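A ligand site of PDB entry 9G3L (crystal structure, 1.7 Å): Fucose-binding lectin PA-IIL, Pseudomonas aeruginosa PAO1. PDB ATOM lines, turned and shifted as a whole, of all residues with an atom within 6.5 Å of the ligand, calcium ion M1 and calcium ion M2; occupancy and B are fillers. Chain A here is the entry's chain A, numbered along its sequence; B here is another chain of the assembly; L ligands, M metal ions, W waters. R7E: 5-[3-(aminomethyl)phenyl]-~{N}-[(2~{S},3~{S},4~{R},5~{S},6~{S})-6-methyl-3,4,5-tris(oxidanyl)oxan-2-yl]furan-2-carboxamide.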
ATOM      1  N   ASN A  21      21.876  -0.742  13.920  1.00  0.00           N
ATOM      2  CA  ASN A  21      20.719  -1.579  13.581  1.00  0.00           C
ATOM      3  C   ASN A  21      19.468  -0.892  14.161  1.00  0.00           C
ATOM      4  O   ASN A  21      18.861  -1.392  15.098  1.00  0.00           O
ATOM      5  CB  ASN A  21      20.854  -2.983  14.116  1.00  0.00           C
ATOM      6  CG  ASN A  21      21.946  -3.801  13.456  1.00  0.00           C
ATOM      7  OD1 ASN A  21      21.731  -4.314  12.348  1.00  0.00           O
ATOM      8  ND2 ASN A  21      23.086  -3.938  14.130  1.00  0.00           N
ATOM      9  N   SER A  22      19.098   0.244  13.593  1.00  0.00           N
ATOM     10  CA  SER A  22      18.017   1.077  14.085  1.00  0.00           C
ATOM     11  C   SER A  22      17.585   2.082  13.022  1.00  0.00           C
ATOM     12  O   SER A  22      18.423   2.483  12.221  1.00  0.00           O
ATOM     13  CB  SER A  22      18.393   1.864  15.338  1.00  0.00           C
ATOM     14  OG  SER A  22      17.306   2.699  15.761  1.00  0.00           O
ATOM     15  N   SER A  23      16.307   2.491  13.040  1.00  0.00           N
ATOM     16  CA  SER A  23      15.811   3.524  12.137  1.00  0.00           C
ATOM     17  C   SER A  23      16.310   4.898  12.553  1.00  0.00           C
ATOM     18  O   SER A  23      16.172   5.842  11.789  1.00  0.00           O
ATOM     19  CB  SER A  23      14.269   3.482  12.089  1.00  0.00           C
ATOM     20  OG  SER A  23      13.684   3.722  13.370  1.00  0.00           O
ATOM     21  N   GLY A  24      16.820   5.010  13.782  1.00  0.00           N
ATOM     22  CA  GLY A  24      17.331   6.286  14.289  1.00  0.00           C
ATOM     23  C   GLY A  24      18.846   6.390  14.128  1.00  0.00           C
ATOM     24  O   GLY A  24      19.565   5.391  14.329  1.00  0.00           O
ATOM     25  N   THR A  25      19.343   7.600  13.804  1.00  0.00           N
ATOM     26  CA  THR A  25      20.794   7.831  13.818  1.00  0.00           C
ATOM     27  C   THR A  25      21.368   7.579  15.209  1.00  0.00           C
ATOM     28  O   THR A  25      20.907   8.181  16.171  1.00  0.00           O
ATOM     29  CB  THR A  25      21.096   9.255  13.313  1.00  0.00           C
ATOM     30  OG1 THR A  25      20.779   9.281  11.918  1.00  0.00           O
ATOM     31  CG2 THR A  25      22.573   9.595  13.383  1.00  0.00           C
ATOM     32  N   GLN A  26      22.433   6.737  15.289  1.00  0.00           N
ATOM     33  CA  GLN A  26      23.114   6.444  16.522  1.00  0.00           C
ATOM     34  C   GLN A  26      24.305   7.367  16.715  1.00  0.00           C
ATOM     35  O   GLN A  26      25.001   7.633  15.737  1.00  0.00           O
ATOM     36  CB  GLN A  26      23.660   5.021  16.413  1.00  0.00           C
ATOM     37  CG  GLN A  26      22.593   3.980  16.157  1.00  0.00           C
ATOM     38  CD  GLN A  26      21.577   3.867  17.259  1.00  0.00           C
ATOM     39  OE1 GLN A  26      21.951   3.629  18.425  1.00  0.00           O
ATOM     40  NE2 GLN A  26      20.290   4.130  16.949  1.00  0.00           N
ATOM     41  N   SER A  44      21.784   2.796  10.190  1.00  0.00           N
ATOM     42  CA  SER A  44      21.600   1.630   9.393  1.00  0.00           C
ATOM     43  C   SER A  44      20.610   0.719  10.089  1.00  0.00           C
ATOM     44  O   SER A  44      20.653   0.624  11.315  1.00  0.00           O
ATOM     45  CB  SER A  44      22.962   0.925   9.165  1.00  0.00           C
ATOM     46  OG  SER A  44      22.786  -0.236   8.347  1.00  0.00           O
ATOM     47  N   THR A  45      19.883  -0.085   9.292  1.00  0.00           N
ATOM     48  CA  THR A  45      19.111  -1.194   9.802  1.00  0.00           C
ATOM     49  C   THR A  45      19.716  -2.487   9.254  1.00  0.00           C
ATOM     50  O   THR A  45      19.059  -3.522   9.301  1.00  0.00           O
ATOM     51  CB  THR A  45      17.624  -1.087   9.445  1.00  0.00           C
ATOM     52  OG1 THR A  45      17.541  -0.766   8.066  1.00  0.00           O
ATOM     53  CG2 THR A  45      16.991  -0.022  10.311  1.00  0.00           C
ATOM     54  N   VAL A  69      20.685   8.570  21.244  1.00  0.00           N
ATOM     55  CA  VAL A  69      19.916   8.701  20.017  1.00  0.00           C
ATOM     56  C   VAL A  69      19.020   9.941  20.195  1.00  0.00           C
ATOM     57  O   VAL A  69      18.264  10.024  21.156  1.00  0.00           O
ATOM     58  CB  VAL A  69      19.087   7.436  19.687  1.00  0.00           C
ATOM     59  CG1 VAL A  69      18.309   7.632  18.396  1.00  0.00           C
ATOM     60  CG2 VAL A  69      19.945   6.198  19.595  1.00  0.00           C
ATOM     61  N   ASN A  70      19.165  10.933  19.315  1.00  0.00           N
ATOM     62  CA  ASN A  70      18.441  12.187  19.415  1.00  0.00           C
ATOM     63  C   ASN A  70      18.605  12.810  20.806  1.00  0.00           C
ATOM     64  O   ASN A  70      17.647  13.384  21.369  1.00  0.00           O
ATOM     65  CB  ASN A  70      16.956  11.979  19.039  1.00  0.00           C
ATOM     66  CG  ASN A  70      16.396  13.266  18.509  1.00  0.00           C
ATOM     67  OD1 ASN A  70      17.117  13.905  17.740  1.00  0.00           O
ATOM     68  ND2 ASN A  70      15.230  13.716  18.986  1.00  0.00           N
ATOM     69  N   ARG A  72      19.075  11.240  23.697  1.00  0.00           N
ATOM     70  CA  ARG A  72      18.677  10.402  24.842  1.00  0.00           C
ATOM     71  C   ARG A  72      19.674   9.231  24.943  1.00  0.00           C
ATOM     72  O   ARG A  72      19.813   8.463  23.999  1.00  0.00           O
ATOM     73  CB  ARG A  72      17.271   9.827  24.636  1.00  0.00           C
ATOM     74  CG  ARG A  72      16.906   8.833  25.754  1.00  0.00           C
ATOM     75  CD  ARG A  72      15.459   8.547  25.976  1.00  0.00           C
ATOM     76  NE  ARG A  72      14.895   7.889  24.795  1.00  0.00           N
ATOM     77  CZ  ARG A  72      13.823   8.289  24.084  1.00  0.00           C
ATOM     78  NH1 ARG A  72      13.710   7.901  22.805  1.00  0.00           N
ATOM     79  NH2 ARG A  72      12.960   9.128  24.612  1.00  0.00           N
ATOM     80  N   SER A  94      23.097  -1.804  22.793  1.00  0.00           N
ATOM     81  CA  SER A  94      22.341  -0.628  23.199  1.00  0.00           C
ATOM     82  C   SER A  94      20.894  -0.745  22.737  1.00  0.00           C
ATOM     83  O   SER A  94      20.645  -1.282  21.650  1.00  0.00           O
ATOM     84  CB  SER A  94      23.019   0.622  22.637  1.00  0.00           C
ATOM     85  OG  SER A  94      22.995   0.711  21.265  1.00  0.00           O
ATOM     86  N   GLU A  95      19.952  -0.176  23.510  1.00  0.00           N
ATOM     87  CA  GLU A  95      18.537  -0.191  23.158  1.00  0.00           C
ATOM     88  C   GLU A  95      18.016   1.249  23.124  1.00  0.00           C
ATOM     89  O   GLU A  95      18.123   1.928  24.137  1.00  0.00           O
ATOM     90  CB  GLU A  95      17.706  -1.041  24.126  1.00  0.00           C
ATOM     91  CG  GLU A  95      16.218  -1.125  23.780  1.00  0.00           C
ATOM     92  CD  GLU A  95      15.926  -1.527  22.365  1.00  0.00           C
ATOM     93  OE1 GLU A  95      16.449  -2.590  21.880  1.00  0.00           O
ATOM     94  OE2 GLU A  95      15.175  -0.778  21.690  1.00  0.00           O
ATOM     95  N   ASP A  96      17.409   1.653  22.019  1.00  0.00           N
ATOM     96  CA  ASP A  96      16.938   3.036  21.842  1.00  0.00           C
ATOM     97  C   ASP A  96      15.410   3.095  21.810  1.00  0.00           C
ATOM     98  O   ASP A  96      14.853   4.147  21.534  1.00  0.00           O
ATOM     99  CB  ASP A  96      17.561   3.652  20.589  1.00  0.00           C
ATOM    100  CG  ASP A  96      17.185   2.995  19.275  1.00  0.00           C
ATOM    101  OD1 ASP A  96      16.214   2.201  19.266  1.00  0.00           O
ATOM    102  OD2 ASP A  96      17.808   3.316  18.251  1.00  0.00           O
ATOM    103  N   GLY A  97      14.750   1.951  21.990  1.00  0.00           N
ATOM    104  CA  GLY A  97      13.301   1.872  21.775  1.00  0.00           C
ATOM    105  C   GLY A  97      12.636   0.882  22.724  1.00  0.00           C
ATOM    106  O   GLY A  97      12.990   0.806  23.910  1.00  0.00           O
ATOM    107  N   THR A  98      11.670   0.118  22.203  1.00  0.00           N
ATOM    108  CA  THR A  98      10.815  -0.726  22.998  1.00  0.00           C
ATOM    109  C   THR A  98      10.952  -2.218  22.687  1.00  0.00           C
ATOM    110  O   THR A  98      10.420  -2.996  23.424  1.00  0.00           O
ATOM    111  CB  THR A  98       9.358  -0.302  22.780  1.00  0.00           C
ATOM    112  OG1 THR A  98       9.135  -0.397  21.379  1.00  0.00           O
ATOM    113  CG2 THR A  98       9.143   1.134  23.211  1.00  0.00           C
ATOM    114  N   ASP A  99      11.684  -2.609  21.640  1.00  0.00           N
ATOM    115  CA  ASP A  99      11.691  -4.018  21.206  1.00  0.00           C
ATOM    116  C   ASP A  99      12.710  -4.861  21.948  1.00  0.00           C
ATOM    117  O   ASP A  99      12.644  -6.077  21.848  1.00  0.00           O
ATOM    118  CB  ASP A  99      11.835  -4.130  19.683  1.00  0.00           C
ATOM    119  CG  ASP A  99      13.182  -3.713  19.131  1.00  0.00           C
ATOM    120  OD1 ASP A  99      13.921  -3.018  19.837  1.00  0.00           O
ATOM    121  OD2 ASP A  99      13.445  -4.033  17.958  1.00  0.00           O
ATOM    122  N   ASN A 100      13.680  -4.222  22.615  1.00  0.00           N
ATOM    123  CA  ASN A 100      14.644  -4.931  23.430  1.00  0.00           C
ATOM    124  C   ASN A 100      15.475  -5.904  22.618  1.00  0.00           C
ATOM    125  O   ASN A 100      15.789  -7.004  23.069  1.00  0.00           O
ATOM    126  CB  ASN A 100      13.969  -5.593  24.642  1.00  0.00           C
ATOM    127  CG  ASN A 100      13.406  -4.542  25.569  1.00  0.00           C
ATOM    128  OD1 ASN A 100      13.926  -3.418  25.627  1.00  0.00           O
ATOM    129  ND2 ASN A 100      12.296  -4.845  26.200  1.00  0.00           N
ATOM    130  N   ASP A 101      15.869  -5.487  21.409  1.00  0.00           N
ATOM    131  CA  ASP A 101      16.813  -6.265  20.623  1.00  0.00           C
ATOM    132  C   ASP A 101      18.237  -5.926  21.060  1.00  0.00           C
ATOM    133  O   ASP A 101      19.160  -6.706  20.769  1.00  0.00           O
ATOM    134  CB  ASP A 101      16.523  -6.179  19.137  1.00  0.00           C
ATOM    135  CG  ASP A 101      16.705  -4.874  18.417  1.00  0.00           C
ATOM    136  OD1 ASP A 101      16.967  -3.854  19.098  1.00  0.00           O
ATOM    137  OD2 ASP A 101      16.601  -4.907  17.147  1.00  0.00           O
ATOM    138  N   TYR A 102      18.427  -4.764  21.678  1.00  0.00           N
ATOM    139  CA  TYR A 102      19.750  -4.335  22.184  1.00  0.00           C
ATOM    140  C   TYR A 102      20.867  -4.352  21.105  1.00  0.00           C
ATOM    141  O   TYR A 102      22.039  -4.407  21.440  1.00  0.00           O
ATOM    142  CB  TYR A 102      20.080  -5.175  23.423  1.00  0.00           C
ATOM    143  CG  TYR A 102      19.454  -4.557  24.657  1.00  0.00           C
ATOM    144  CD1 TYR A 102      18.139  -4.845  24.995  1.00  0.00           C
ATOM    145  CD2 TYR A 102      20.123  -3.593  25.391  1.00  0.00           C
ATOM    146  CE1 TYR A 102      17.535  -4.279  26.102  1.00  0.00           C
ATOM    147  CE2 TYR A 102      19.516  -2.977  26.471  1.00  0.00           C
ATOM    148  CZ  TYR A 102      18.217  -3.288  26.794  1.00  0.00           C
ATOM    149  OH  TYR A 102      17.584  -2.703  27.866  1.00  0.00           O
ATOM    150  N   ASN A 103      20.516  -4.095  19.844  1.00  0.00           N
ATOM    151  CA  ASN A 103      21.490  -4.088  18.758  1.00  0.00           C
ATOM    152  C   ASN A 103      21.520  -2.747  18.052  1.00  0.00           C
ATOM    153  O   ASN A 103      22.123  -2.631  16.993  1.00  0.00           O
ATOM    154  CB  ASN A 103      21.188  -5.216  17.763  1.00  0.00           C
ATOM    155  CG  ASN A 103      19.998  -4.880  16.871  1.00  0.00           C
ATOM    156  OD1 ASN A 103      19.295  -3.901  17.130  1.00  0.00           O
ATOM    157  ND2 ASN A 103      19.696  -5.737  15.939  1.00  0.00           N
ATOM    158  N   ASP A 104      20.835  -1.748  18.630  1.00  0.00           N
ATOM    159  CA  ASP A 104      20.621  -0.473  17.956  1.00  0.00           C
ATOM    160  C   ASP A 104      21.946   0.178  17.587  1.00  0.00           C
ATOM    161  O   ASP A 104      22.130   0.637  16.455  1.00  0.00           O
ATOM    162  CB  ASP A 104      19.605   0.318  18.763  1.00  0.00           C
ATOM    163  CG  ASP A 104      18.283  -0.397  18.927  1.00  0.00           C
ATOM    164  OD1 ASP A 104      17.892  -1.088  17.970  1.00  0.00           O
ATOM    165  OD2 ASP A 104      17.671  -0.314  20.028  1.00  0.00           O
ATOM    166  N   LEU B 113      20.236  -8.724  13.718  1.00  0.00           N
ATOM    167  CA  LEU B 113      20.372  -7.463  12.995  1.00  0.00           C
ATOM    168  C   LEU B 113      19.006  -6.776  12.905  1.00  0.00           C
ATOM    169  O   LEU B 113      17.969  -7.380  13.252  1.00  0.00           O
ATOM    170  CB  LEU B 113      20.920  -7.725  11.583  1.00  0.00           C
ATOM    171  CG  LEU B 113      22.209  -8.523  11.452  1.00  0.00           C
ATOM    172  CD1 LEU B 113      22.789  -8.431  10.013  1.00  0.00           C
ATOM    173  CD2 LEU B 113      23.223  -8.020  12.422  1.00  0.00           C
ATOM    174  N   GLY B 114      19.025  -5.552  12.385  1.00  0.00           N
ATOM    175  CA  GLY B 114      17.785  -4.862  12.082  1.00  0.00           C
ATOM    176  C   GLY B 114      17.270  -3.960  13.198  1.00  0.00           C
ATOM    177  O   GLY B 114      17.662  -4.150  14.358  1.00  0.00           O
ATOM    178  OXT GLY B 114      16.472  -3.064  12.817  1.00  0.00           O
HETATM  179  N1  R7E L   1      14.499   2.436  16.645  1.00  0.00           N
HETATM  180  C4  R7E L   1      14.600  -1.517  15.114  1.00  0.00           C
HETATM  181  C5  R7E L   1      13.934  -0.353  14.378  1.00  0.00           C
HETATM  182  C6  R7E L   1      14.195  -0.437  12.894  1.00  0.00           C
HETATM  183  C7  R7E L   1      13.579   3.416  16.578  1.00  0.00           C
HETATM  184  C8  R7E L   1      14.020   4.746  16.884  1.00  0.00           C
HETATM  185  C10 R7E L   1      14.964   6.739  17.325  1.00  0.00           C
HETATM  186  C13 R7E L   1      11.382   7.928  17.079  1.00  0.00           C
HETATM  187  C15 R7E L   1      11.075  10.322  17.049  1.00  0.00           C
HETATM  188  C17 R7E L   1      13.306   9.389  17.053  1.00  0.00           C
HETATM  189  C1  R7E L   1      14.158   1.109  16.269  1.00  0.00           C
HETATM  190  O5  R7E L   1      14.417   0.920  14.860  1.00  0.00           O
HETATM  191  C3  R7E L   1      14.472  -1.318  16.620  1.00  0.00           C
HETATM  192  O3  R7E L   1      15.202  -2.365  17.286  1.00  0.00           O
HETATM  193  C2  R7E L   1      14.971   0.056  17.036  1.00  0.00           C
HETATM  194  O2  R7E L   1      14.807   0.189  18.455  1.00  0.00           O
HETATM  195  O4  R7E L   1      15.976  -1.589  14.786  1.00  0.00           O
HETATM  196  O7  R7E L   1      12.414   3.186  16.218  1.00  0.00           O
HETATM  197  O8  R7E L   1      13.053   5.715  16.763  1.00  0.00           O
HETATM  198  C11 R7E L   1      13.645   6.932  17.055  1.00  0.00           C
HETATM  199  C9  R7E L   1      15.203   5.344  17.168  1.00  0.00           C
HETATM  200  C12 R7E L   1      12.768   8.094  17.053  1.00  0.00           C
HETATM  201  C16 R7E L   1      12.461  10.478  17.065  1.00  0.00           C
HETATM  202  C14 R7E L   1      10.529   9.038  17.068  1.00  0.00           C
HETATM  203  C18 R7E L   1       9.031   8.843  17.124  1.00  0.00           C
HETATM  204  N2  R7E L   1       8.426   8.889  15.818  1.00  0.00           N
HETATM  205 CA    CA M   1      15.919  -1.828  19.628  1.00  0.00          CA
HETATM  206 CA    CA M   2      17.448  -2.779  16.412  1.00  0.00          CA
HETATM  207  O   HOH W   1       5.864   9.491  16.626  1.00  0.00           O
HETATM  208  O   HOH W   2       8.015   5.827  15.595  1.00  0.00           O
HETATM  209  O   HOH W   3      10.496   4.958  15.081  1.00  0.00           O
HETATM  210  O   HOH W   4      11.489   1.981  13.390  1.00  0.00           O
HETATM  211  O   HOH W   5      12.086  -0.289  19.322  1.00  0.00           O
HETATM  212  O   HOH W   6      10.934   3.193  18.877  1.00  0.00           O
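CA of Gly 24 touches C9 of the ligand, 3.7 Å away.
Thr 45 touches the ligand (CG2 to C6, 3.8 Å).
CG1 of Val 69 touches C10 of the ligand, 3.6 Å away.
Gly 97 touches the ligand (N to O2, 3.95 Å).
Hydrophobic or aromatic side chains within 4 Å of the ligand: Val 69.
The nearest printed residue that does not touch the ligand is Asn 103 (4.4 Å).
Five residues have an atom within 4 Å of calcium ion M2: Asn 21, Asp 101, Asn 103, Asp 104 and Gly 114 of chain B.
The nearest printed residue that does not touch calcium ion M2 is Ser 22 (4.5 Å).
Four residues have an atom within 4 Å of calcium ion M1: Glu 95, Asp 99, Asp 101 and Asp 104.
The side-chain carboxylate (OD1) of Asp 96 sits at hydrogen-bond distance from a nitrogen (N1) of the ligand (3.1 Å).
N1 of the ligand is in hydrogen-bond range of OG of Ser 22 (3.0 Å).
N of Ser 23 sits at hydrogen-bond distance from O5 of the ligand (3.1 Å).
The side-chain hydroxyl (OG) of Ser 23 lies within hydrogen-bond range of an oxygen (O7) of the ligand (3.2 Å).
O of Ser 94 lies within hydrogen-bond range of N of Asn 103, at 3.3 Å.
The backbone NH (N) of Asn 21 sits close to the backbone carbonyl oxygen (O) of Ser 44 (3.2 Å).
OE2 of Glu 95 lies close to N of Gly 97, 2.8 Å away.
The side-chain carboxylate (OE1) of Glu 95 lies close to the backbone NH (N) of Asn 100 (3.3 Å).
The side-chain hydroxyl of Ser 22 is in hydrogen-bond range of the side-chain carboxylate of Asp 96, 2.6 Å away.
OG of Ser 22 is in hydrogen-bond range of N of Gly 24 (3.1 Å).
The backbone NH of Ser 22 lies within hydrogen-bond range of the backbone carbonyl oxygen of Ser 44 (2.8 Å).
The backbone carbonyl oxygen (O) of Gly 24 is in hydrogen-bond range of the side-chain amide nitrogen (NE2) of Gln 26, 3.0 Å away.
Calcium ion M2 is bound by OD1 of Asn 103, OD1 of Asp 104, O of Asn 21, OD2 of Asp 101, O3 of the ligand, O of Gly 114 of chain B and O4 of the ligand.
Slightly farther from calcium ion M2 lies OD1 of Asp 101 (2.9 Å).
Water W4 bridges OG of Ser 23 (2.8 Å) and O7 of the ligand (3.2 Å).
Calcium ion M1 is bound by the side-chain carboxylate (OD1) of Asp 99 (2.3 Å), the side-chain carboxylate (OD1) of Asp 101 (2.3 Å), the side-chain carboxylate (OD2) of Asp 104 (2.3 Å), the side-chain carboxylate (OE2) of Glu 95 (2.4 Å), the side-chain carboxylate (OE1) of Glu 95 (2.4 Å), an oxygen (O3) of the ligand (2.5 Å), an oxygen (O2) of the ligand (2.6 Å) and the side-chain carboxylate (OD1) of Asp 104 (2.7 Å).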
